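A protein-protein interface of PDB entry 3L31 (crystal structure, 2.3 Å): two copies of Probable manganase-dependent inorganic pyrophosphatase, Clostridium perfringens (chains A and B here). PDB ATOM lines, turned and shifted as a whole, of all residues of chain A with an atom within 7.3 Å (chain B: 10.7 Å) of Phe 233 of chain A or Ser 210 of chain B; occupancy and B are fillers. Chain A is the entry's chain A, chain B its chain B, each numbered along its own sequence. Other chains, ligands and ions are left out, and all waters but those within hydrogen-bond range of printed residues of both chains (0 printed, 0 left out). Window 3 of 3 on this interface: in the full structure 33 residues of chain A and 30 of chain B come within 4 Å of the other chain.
OD1 of Asp 12 of chain A is in hydrogen-bond range of NE2 of His 234 of chain A (3.5 Å).
The backbone NH (N) of Ala 231 of chain A sits at hydrogen-bond distance from a ring nitrogen (ND1) of His 234 of chain A, at 3.1 Å.
The backbone carbonyl oxygen (O) of Val 207 of chain B sits at hydrogen-bond distance from the side-chain hydroxyl (OG) of Ser 210 of chain B (2.7 Å).
Among the printed residues, pairs that only touch across the chains: Ala 231 of chain A with Arg 213 of chain B, Phe 233 of chain A with Ser 210 of chain B, Phe 233 of chain A with Arg 213 of chain B and His 234 of chain A with Arg 213 of chain B.
Of the printed residues of chain B, Phe 233 of chain A touches Ser 210 and Arg 213.
Ala 231 of chain A touches just one residue of chain B: Arg 213.
Of chain B, only Arg 213 (3.7 Å) comes within 4 Å of His 234 of chain A.
Leu 235 of chain A touches none of the printed residues of chain B.
Printed residues of chain A within 4 Å of Arg 213 of chain B: Ala 231, Phe 233 and His 234.
Ser 215 of chain B touches none of the printed residues of chain A.
Hydrophobic or aromatic side chains of chain A that line the printed part of chain B: Ala 231, Phe 233 and His 234.
Of the 21 printed residues of chain B, 2 touch a printed residue of chain A.
Among the printed residues, 4 pairs touch across the chains.
Positions printed for both chains: 209, 215, 230, 231, 232 and 233.
Of the 4 pairs that touch across the chains among the printed residues, none has its exchanged pair printed and touching as well.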
ATOM      1  N   GLU A  10      -4.581   2.977  14.492  1.00  0.00           N
ATOM      2  CA  GLU A  10      -5.055   3.580  13.236  1.00  0.00           C
ATOM      3  C   GLU A  10      -6.470   3.090  12.988  1.00  0.00           C
ATOM      4  O   GLU A  10      -6.686   1.913  12.721  1.00  0.00           O
ATOM      5  CB  GLU A  10      -4.145   3.231  12.037  1.00  0.00           C
ATOM      6  CG  GLU A  10      -4.252   4.220  10.834  1.00  0.00           C
ATOM      7  CD  GLU A  10      -3.119   4.062   9.789  1.00  0.00           C
ATOM      8  OE1 GLU A  10      -2.065   3.462  10.101  1.00  0.00           O
ATOM      9  OE2 GLU A  10      -3.287   4.547   8.647  1.00  0.00           O
ATOM     10  N   ASP A  12     -10.913   4.080  11.941  1.00  0.00           N
ATOM     11  CA  ASP A  12     -11.803   4.756  10.984  1.00  0.00           C
ATOM     12  C   ASP A  12     -12.309   6.090  11.555  1.00  0.00           C
ATOM     13  O   ASP A  12     -13.157   6.115  12.460  1.00  0.00           O
ATOM     14  CB  ASP A  12     -12.972   3.847  10.583  1.00  0.00           C
ATOM     15  CG  ASP A  12     -12.530   2.628   9.747  1.00  0.00           C
ATOM     16  OD1 ASP A  12     -11.366   2.581   9.264  1.00  0.00           O
ATOM     17  OD2 ASP A  12     -13.354   1.705   9.576  1.00  0.00           O
ATOM     18  N   MET A 209     -14.091  -5.870  23.965  1.00  0.00           N
ATOM     19  CA  MET A 209     -14.543  -6.331  22.661  1.00  0.00           C
ATOM     20  C   MET A 209     -14.921  -7.807  22.655  1.00  0.00           C
ATOM     21  O   MET A 209     -15.768  -8.225  21.850  1.00  0.00           O
ATOM     22  CB  MET A 209     -13.481  -6.100  21.582  1.00  0.00           C
ATOM     23  CG  MET A 209     -13.296  -4.632  21.195  1.00  0.00           C
ATOM     24  SD  MET A 209     -12.541  -4.420  19.543  1.00  0.00           S
ATOM     25  CE  MET A 209     -12.365  -2.633  19.490  1.00  0.00           C
ATOM     26  N   SER A 215     -19.724  -5.215  15.196  1.00  0.00           N
ATOM     27  CA  SER A 215     -18.745  -4.961  14.129  1.00  0.00           C
ATOM     28  C   SER A 215     -17.827  -3.822  14.525  1.00  0.00           C
ATOM     29  O   SER A 215     -16.622  -3.933  14.437  1.00  0.00           O
ATOM     30  CB  SER A 215     -19.426  -4.666  12.785  1.00  0.00           C
ATOM     31  OG  SER A 215     -20.184  -5.766  12.267  1.00  0.00           O
ATOM     32  N   ILE A 230     -13.738   1.908  15.931  1.00  0.00           N
ATOM     33  CA  ILE A 230     -12.726   0.871  15.884  1.00  0.00           C
ATOM     34  C   ILE A 230     -13.305  -0.525  15.709  1.00  0.00           C
ATOM     35  O   ILE A 230     -14.389  -0.836  16.183  1.00  0.00           O
ATOM     36  CB  ILE A 230     -11.917   0.876  17.197  1.00  0.00           C
ATOM     37  CG1 ILE A 230     -10.740   1.825  17.083  1.00  0.00           C
ATOM     38  CG2 ILE A 230     -11.302  -0.466  17.456  1.00  0.00           C
ATOM     39  CD1 ILE A 230      -9.454   1.091  16.698  1.00  0.00           C
ATOM     40  N   ALA A 231     -12.560  -1.389  15.049  1.00  0.00           N
ATOM     41  CA  ALA A 231     -12.975  -2.785  14.970  1.00  0.00           C
ATOM     42  C   ALA A 231     -11.850  -3.681  15.425  1.00  0.00           C
ATOM     43  O   ALA A 231     -10.721  -3.240  15.567  1.00  0.00           O
ATOM     44  CB  ALA A 231     -13.427  -3.127  13.574  1.00  0.00           C
ATOM     45  N   ARG A 232     -12.206  -4.927  15.715  1.00  0.00           N
ATOM     46  CA  ARG A 232     -11.250  -5.974  16.067  1.00  0.00           C
ATOM     47  C   ARG A 232     -10.056  -5.913  15.116  1.00  0.00           C
ATOM     48  O   ARG A 232      -8.917  -6.152  15.505  1.00  0.00           O
ATOM     49  CB  ARG A 232     -11.906  -7.374  16.039  1.00  0.00           C
ATOM     50  CG  ARG A 232     -12.660  -7.713  17.319  1.00  0.00           C
ATOM     51  CD  ARG A 232     -13.609  -8.908  17.212  1.00  0.00           C
ATOM     52  NE  ARG A 232     -14.693  -8.812  18.201  1.00  0.00           N
ATOM     53  CZ  ARG A 232     -15.836  -8.135  17.989  1.00  0.00           C
ATOM     54  NH1 ARG A 232     -16.041  -7.518  16.823  1.00  0.00           N
ATOM     55  NH2 ARG A 232     -16.778  -8.057  18.931  1.00  0.00           N
ATOM     56  N   PHE A 233     -10.343  -5.542  13.874  1.00  0.00           N
ATOM     57  CA  PHE A 233      -9.346  -5.518  12.789  1.00  0.00           C
ATOM     58  C   PHE A 233      -8.221  -4.512  13.012  1.00  0.00           C
ATOM     59  O   PHE A 233      -7.149  -4.648  12.455  1.00  0.00           O
ATOM     60  CB  PHE A 233     -10.017  -5.224  11.432  1.00  0.00           C
ATOM     61  CG  PHE A 233      -9.034  -4.950  10.311  1.00  0.00           C
ATOM     62  CD1 PHE A 233      -8.568  -5.987   9.497  1.00  0.00           C
ATOM     63  CD2 PHE A 233      -8.578  -3.661  10.060  1.00  0.00           C
ATOM     64  CE1 PHE A 233      -7.668  -5.742   8.451  1.00  0.00           C
ATOM     65  CE2 PHE A 233      -7.666  -3.408   9.012  1.00  0.00           C
ATOM     66  CZ  PHE A 233      -7.222  -4.450   8.210  1.00  0.00           C
ATOM     67  N   HIS A 234      -8.481  -3.495  13.815  1.00  0.00           N
ATOM     68  CA  HIS A 234      -7.507  -2.430  14.040  1.00  0.00           C
ATOM     69  C   HIS A 234      -6.638  -2.826  15.220  1.00  0.00           C
ATOM     70  O   HIS A 234      -5.828  -2.034  15.708  1.00  0.00           O
ATOM     71  CB  HIS A 234      -8.196  -1.097  14.332  1.00  0.00           C
ATOM     72  CG  HIS A 234      -8.961  -0.532  13.177  1.00  0.00           C
ATOM     73  ND1 HIS A 234     -10.333  -0.398  13.190  1.00  0.00           N
ATOM     74  CD2 HIS A 234      -8.547  -0.042  11.986  1.00  0.00           C
ATOM     75  CE1 HIS A 234     -10.731   0.144  12.053  1.00  0.00           C
ATOM     76  NE2 HIS A 234      -9.669   0.370  11.305  1.00  0.00           N
ATOM     77  N   LEU A 235      -6.836  -4.066  15.664  1.00  0.00           N
ATOM     78  CA  LEU A 235      -6.044  -4.675  16.752  1.00  0.00           C
ATOM     79  C   LEU A 235      -5.127  -5.786  16.222  1.00  0.00           C
ATOM     80  O   LEU A 235      -3.904  -5.665  16.277  1.00  0.00           O
ATOM     81  CB  LEU A 235      -6.963  -5.256  17.849  1.00  0.00           C
ATOM     82  CG  LEU A 235      -8.129  -4.375  18.345  1.00  0.00           C
ATOM     83  CD1 LEU A 235      -8.983  -5.135  19.349  1.00  0.00           C
ATOM     84  CD2 LEU A 235      -7.643  -3.065  18.957  1.00  0.00           C
ATOM     85  N   VAL B 194     -13.331 -16.758   0.673  1.00  0.00           N
ATOM     86  CA  VAL B 194     -12.214 -17.082   1.543  1.00  0.00           C
ATOM     87  C   VAL B 194     -12.637 -18.011   2.664  1.00  0.00           C
ATOM     88  O   VAL B 194     -13.371 -17.628   3.589  1.00  0.00           O
ATOM     89  CB  VAL B 194     -11.527 -15.840   2.088  1.00  0.00           C
ATOM     90  CG1 VAL B 194     -10.264 -16.253   2.817  1.00  0.00           C
ATOM     91  CG2 VAL B 194     -11.207 -14.881   0.945  1.00  0.00           C
ATOM     92  N   VAL B 196     -11.514 -21.576   5.264  1.00  0.00           N
ATOM     93  CA  VAL B 196     -10.514 -22.028   6.219  1.00  0.00           C
ATOM     94  C   VAL B 196     -10.768 -23.472   6.575  1.00  0.00           C
ATOM     95  O   VAL B 196     -11.902 -23.845   6.882  1.00  0.00           O
ATOM     96  CB  VAL B 196     -10.580 -21.181   7.508  1.00  0.00           C
ATOM     97  CG1 VAL B 196     -10.300 -22.026   8.720  1.00  0.00           C
ATOM     98  CG2 VAL B 196      -9.611 -20.014   7.437  1.00  0.00           C
ATOM     99  N   VAL B 202      -3.818 -21.921  13.454  1.00  0.00           N
ATOM    100  CA  VAL B 202      -4.610 -20.798  13.900  1.00  0.00           C
ATOM    101  C   VAL B 202      -3.811 -19.519  13.667  1.00  0.00           C
ATOM    102  O   VAL B 202      -4.369 -18.441  13.462  1.00  0.00           O
ATOM    103  CB  VAL B 202      -5.022 -20.926  15.381  1.00  0.00           C
ATOM    104  CG1 VAL B 202      -5.322 -19.548  15.982  1.00  0.00           C
ATOM    105  CG2 VAL B 202      -6.204 -21.850  15.500  1.00  0.00           C
ATOM    106  N   GLU B 203      -2.492 -19.654  13.691  1.00  0.00           N
ATOM    107  CA  GLU B 203      -1.598 -18.510  13.478  1.00  0.00           C
ATOM    108  C   GLU B 203      -1.626 -18.139  11.991  1.00  0.00           C
ATOM    109  O   GLU B 203      -1.349 -17.003  11.623  1.00  0.00           O
ATOM    110  CB  GLU B 203      -0.159 -18.810  13.957  1.00  0.00           C
ATOM    111  N   ASP B 204      -1.993 -19.096  11.144  1.00  0.00           N
ATOM    112  CA  ASP B 204      -1.972 -18.874   9.680  1.00  0.00           C
ATOM    113  C   ASP B 204      -3.285 -18.313   9.156  1.00  0.00           C
ATOM    114  O   ASP B 204      -3.334 -17.664   8.108  1.00  0.00           O
ATOM    115  CB  ASP B 204      -1.610 -20.149   8.910  1.00  0.00           C
ATOM    116  CG  ASP B 204      -0.109 -20.362   8.830  1.00  0.00           C
ATOM    117  OD1 ASP B 204       0.649 -19.433   9.210  1.00  0.00           O
ATOM    118  OD2 ASP B 204       0.308 -21.447   8.389  1.00  0.00           O
ATOM    119  N   VAL B 205      -4.338 -18.571   9.915  1.00  0.00           N
ATOM    120  CA  VAL B 205      -5.657 -18.057   9.601  1.00  0.00           C
ATOM    121  C   VAL B 205      -5.695 -16.610  10.076  1.00  0.00           C
ATOM    122  O   VAL B 205      -6.519 -15.798   9.650  1.00  0.00           O
ATOM    123  CB  VAL B 205      -6.736 -18.905  10.268  1.00  0.00           C
ATOM    124  CG1 VAL B 205      -8.082 -18.295  10.054  1.00  0.00           C
ATOM    125  CG2 VAL B 205      -6.691 -20.317   9.708  1.00  0.00           C
ATOM    126  N   LYS B 206      -4.749 -16.285  10.947  1.00  0.00           N
ATOM    127  CA  LYS B 206      -4.636 -14.927  11.461  1.00  0.00           C
ATOM    128  C   LYS B 206      -4.082 -13.982  10.384  1.00  0.00           C
ATOM    129  O   LYS B 206      -4.573 -12.852  10.218  1.00  0.00           O
ATOM    130  CB  LYS B 206      -3.781 -14.879  12.727  1.00  0.00           C
ATOM    131  CG  LYS B 206      -4.564 -15.140  13.998  1.00  0.00           C
ATOM    132  CD  LYS B 206      -3.646 -15.050  15.212  1.00  0.00           C
ATOM    133  CE  LYS B 206      -4.326 -14.376  16.393  1.00  0.00           C
ATOM    134  NZ  LYS B 206      -3.356 -14.112  17.484  1.00  0.00           N
ATOM    135  N   VAL B 207      -3.054 -14.440   9.666  1.00  0.00           N
ATOM    136  CA  VAL B 207      -2.517 -13.679   8.522  1.00  0.00           C
ATOM    137  C   VAL B 207      -3.589 -13.606   7.435  1.00  0.00           C
ATOM    138  O   VAL B 207      -3.867 -12.536   6.904  1.00  0.00           O
ATOM    139  CB  VAL B 207      -1.200 -14.273   7.942  1.00  0.00           C
ATOM    140  CG1 VAL B 207      -0.909 -13.719   6.550  1.00  0.00           C
ATOM    141  CG2 VAL B 207      -0.035 -13.987   8.876  1.00  0.00           C
ATOM    142  N   THR B 208      -4.205 -14.738   7.124  1.00  0.00           N
ATOM    143  CA  THR B 208      -5.246 -14.757   6.098  1.00  0.00           C
ATOM    144  C   THR B 208      -6.301 -13.700   6.392  1.00  0.00           C
ATOM    145  O   THR B 208      -6.628 -12.866   5.549  1.00  0.00           O
ATOM    146  CB  THR B 208      -5.955 -16.109   6.004  1.00  0.00           C
ATOM    147  OG1 THR B 208      -4.986 -17.149   5.849  1.00  0.00           O
ATOM    148  CG2 THR B 208      -6.909 -16.125   4.801  1.00  0.00           C
ATOM    149  N   MET B 209      -6.818 -13.744   7.610  1.00  0.00           N
ATOM    150  CA  MET B 209      -7.940 -12.883   8.004  1.00  0.00           C
ATOM    151  C   MET B 209      -7.644 -11.382   7.959  1.00  0.00           C
ATOM    152  O   MET B 209      -8.529 -10.574   7.639  1.00  0.00           O
ATOM    153  CB  MET B 209      -8.468 -13.252   9.395  1.00  0.00           C
ATOM    154  CG  MET B 209      -9.406 -14.466   9.391  1.00  0.00           C
ATOM    155  SD  MET B 209     -10.314 -14.666  10.952  1.00  0.00           S
ATOM    156  CE  MET B 209     -10.948 -16.333  10.784  1.00  0.00           C
ATOM    157  N   SER B 210      -6.419 -11.008   8.311  1.00  0.00           N
ATOM    158  CA  SER B 210      -6.022  -9.590   8.360  1.00  0.00           C
ATOM    159  C   SER B 210      -5.990  -8.940   6.978  1.00  0.00           C
ATOM    160  O   SER B 210      -5.858  -7.724   6.857  1.00  0.00           O
ATOM    161  CB  SER B 210      -4.627  -9.465   8.959  1.00  0.00           C
ATOM    162  OG  SER B 210      -3.713 -10.171   8.129  1.00  0.00           O
ATOM    163  N   GLU B 211      -6.066  -9.760   5.943  1.00  0.00           N
ATOM    164  CA  GLU B 211      -5.966  -9.275   4.562  1.00  0.00           C
ATOM    165  C   GLU B 211      -7.350  -8.973   3.994  1.00  0.00           C
ATOM    166  O   GLU B 211      -7.486  -8.527   2.854  1.00  0.00           O
ATOM    167  CB  GLU B 211      -5.226 -10.296   3.672  1.00  0.00           C
ATOM    168  CG  GLU B 211      -3.758 -10.538   4.099  1.00  0.00           C
ATOM    169  CD  GLU B 211      -3.176 -11.849   3.558  1.00  0.00           C
ATOM    170  OE1 GLU B 211      -3.871 -12.513   2.751  1.00  0.00           O
ATOM    171  OE2 GLU B 211      -2.030 -12.213   3.939  1.00  0.00           O
ATOM    172  N   THR B 212      -8.373  -9.225   4.806  1.00  0.00           N
ATOM    173  CA  THR B 212      -9.775  -8.940   4.434  1.00  0.00           C
ATOM    174  C   THR B 212     -10.604  -8.399   5.613  1.00  0.00           C
ATOM    175  O   THR B 212     -10.183  -8.434   6.753  1.00  0.00           O
ATOM    176  CB  THR B 212     -10.459 -10.166   3.775  1.00  0.00           C
ATOM    177  OG1 THR B 212      -9.836 -11.396   4.195  1.00  0.00           O
ATOM    178  CG2 THR B 212     -10.349 -10.060   2.260  1.00  0.00           C
ATOM    179  N   ARG B 213     -11.770  -7.856   5.323  1.00  0.00           N
ATOM    180  CA  ARG B 213     -12.629  -7.316   6.366  1.00  0.00           C
ATOM    181  C   ARG B 213     -13.977  -8.023   6.442  1.00  0.00           C
ATOM    182  O   ARG B 213     -14.997  -7.399   6.703  1.00  0.00           O
ATOM    183  CB  ARG B 213     -12.861  -5.827   6.118  1.00  0.00           C
ATOM    184  CG  ARG B 213     -11.596  -4.969   6.116  1.00  0.00           C
ATOM    185  CD  ARG B 213     -11.086  -4.665   7.534  1.00  0.00           C
ATOM    186  NE  ARG B 213     -12.116  -4.093   8.413  1.00  0.00           N
ATOM    187  CZ  ARG B 213     -12.009  -2.921   9.039  1.00  0.00           C
ATOM    188  NH1 ARG B 213     -10.916  -2.176   8.892  1.00  0.00           N
ATOM    189  NH2 ARG B 213     -12.990  -2.495   9.822  1.00  0.00           N
ATOM    190  N   TYR B 214     -13.993  -9.321   6.193  1.00  0.00           N
ATOM    191  CA  TYR B 214     -15.258 -10.075   6.195  1.00  0.00           C
ATOM    192  C   TYR B 214     -15.689 -10.491   7.604  1.00  0.00           C
ATOM    193  O   TYR B 214     -14.902 -10.982   8.396  1.00  0.00           O
ATOM    194  CB  TYR B 214     -15.164 -11.327   5.292  1.00  0.00           C
ATOM    195  CG  TYR B 214     -14.733 -11.048   3.866  1.00  0.00           C
ATOM    196  CD1 TYR B 214     -15.406 -10.103   3.081  1.00  0.00           C
ATOM    197  CD2 TYR B 214     -13.680 -11.747   3.287  1.00  0.00           C
ATOM    198  CE1 TYR B 214     -15.021  -9.851   1.757  1.00  0.00           C
ATOM    199  CE2 TYR B 214     -13.294 -11.506   1.969  1.00  0.00           C
ATOM    200  CZ  TYR B 214     -13.967 -10.552   1.213  1.00  0.00           C
ATOM    201  OH  TYR B 214     -13.576 -10.298  -0.084  1.00  0.00           O
ATOM    202  N   SER B 215     -16.967 -10.344   7.884  1.00  0.00           N
ATOM    203  CA  SER B 215     -17.477 -10.742   9.184  1.00  0.00           C
ATOM    204  C   SER B 215     -17.192 -12.204   9.499  1.00  0.00           C
ATOM    205  O   SER B 215     -16.744 -12.526  10.578  1.00  0.00           O
ATOM    206  CB  SER B 215     -18.975 -10.496   9.271  1.00  0.00           C
ATOM    207  OG  SER B 215     -19.281  -9.131   9.087  1.00  0.00           O
ATOM    208  N   TYR B 217     -15.876 -16.340   8.020  1.00  0.00           N
ATOM    209  CA  TYR B 217     -15.162 -17.221   7.089  1.00  0.00           C
ATOM    210  C   TYR B 217     -15.684 -18.625   7.304  1.00  0.00           C
ATOM    211  O   TYR B 217     -15.732 -19.104   8.437  1.00  0.00           O
ATOM    212  CB  TYR B 217     -13.634 -17.139   7.343  1.00  0.00           C
ATOM    213  CG  TYR B 217     -13.116 -15.724   7.202  1.00  0.00           C
ATOM    214  CD1 TYR B 217     -12.442 -15.314   6.054  1.00  0.00           C
ATOM    215  CD2 TYR B 217     -13.359 -14.789   8.175  1.00  0.00           C
ATOM    216  CE1 TYR B 217     -11.988 -14.008   5.909  1.00  0.00           C
ATOM    217  CE2 TYR B 217     -12.912 -13.475   8.044  1.00  0.00           C
ATOM    218  CZ  TYR B 217     -12.225 -13.088   6.902  1.00  0.00           C
ATOM    219  OH  TYR B 217     -11.817 -11.779   6.751  1.00  0.00           O
ATOM    220  N   ILE B 230     -16.097 -19.338  11.198  1.00  0.00           N
ATOM    221  CA  ILE B 230     -15.464 -18.605  12.290  1.00  0.00           C
ATOM    222  C   ILE B 230     -15.220 -17.146  11.941  1.00  0.00           C
ATOM    223  O   ILE B 230     -15.250 -16.739  10.770  1.00  0.00           O
ATOM    224  CB  ILE B 230     -14.132 -19.249  12.778  1.00  0.00           C
ATOM    225  CG1 ILE B 230     -13.334 -19.828  11.605  1.00  0.00           C
ATOM    226  CG2 ILE B 230     -14.421 -20.343  13.796  1.00  0.00           C
ATOM    227  CD1 ILE B 230     -12.682 -18.758  10.718  1.00  0.00           C
ATOM    228  N   ALA B 231     -14.974 -16.380  12.994  1.00  0.00           N
ATOM    229  CA  ALA B 231     -14.781 -14.942  12.888  1.00  0.00           C
ATOM    230  C   ALA B 231     -13.614 -14.478  13.732  1.00  0.00           C
ATOM    231  O   ALA B 231     -13.101 -15.208  14.573  1.00  0.00           O
ATOM    232  CB  ALA B 231     -16.027 -14.224  13.287  1.00  0.00           C
ATOM    233  N   ARG B 232     -13.204 -13.248  13.465  1.00  0.00           N
ATOM    234  CA  ARG B 232     -12.129 -12.591  14.222  1.00  0.00           C
ATOM    235  C   ARG B 232     -12.399 -12.778  15.696  1.00  0.00           C
ATOM    236  O   ARG B 232     -11.485 -12.898  16.508  1.00  0.00           O
ATOM    237  CB  ARG B 232     -12.017 -11.085  13.910  1.00  0.00           C
ATOM    238  CG  ARG B 232     -10.964 -10.729  12.840  1.00  0.00           C
ATOM    239  CD  ARG B 232     -11.176  -9.338  12.224  1.00  0.00           C
ATOM    240  NE  ARG B 232     -10.907  -9.376  10.790  1.00  0.00           N
ATOM    241  CZ  ARG B 232     -11.784  -9.829   9.885  1.00  0.00           C
ATOM    242  NH1 ARG B 232     -12.987 -10.255  10.272  1.00  0.00           N
ATOM    243  NH2 ARG B 232     -11.468  -9.867   8.594  1.00  0.00           N
ATOM    244  N   PHE B 233     -13.682 -12.801  16.026  1.00  0.00           N
ATOM    245  CA  PHE B 233     -14.101 -12.960  17.406  1.00  0.00           C
ATOM    246  C   PHE B 233     -13.492 -14.202  17.997  1.00  0.00           C
ATOM    247  O   PHE B 233     -12.987 -14.212  19.106  1.00  0.00           O
ATOM    248  CB  PHE B 233     -15.617 -13.083  17.510  1.00  0.00           C
ATOM    249  CG  PHE B 233     -16.087 -13.379  18.894  1.00  0.00           C
ATOM    250  CD1 PHE B 233     -16.300 -12.345  19.798  1.00  0.00           C
ATOM    251  CD2 PHE B 233     -16.282 -14.678  19.308  1.00  0.00           C
ATOM    252  CE1 PHE B 233     -16.725 -12.605  21.089  1.00  0.00           C
ATOM    253  CE2 PHE B 233     -16.700 -14.947  20.596  1.00  0.00           C
ATOM    254  CZ  PHE B 233     -16.924 -13.916  21.487  1.00  0.00           C
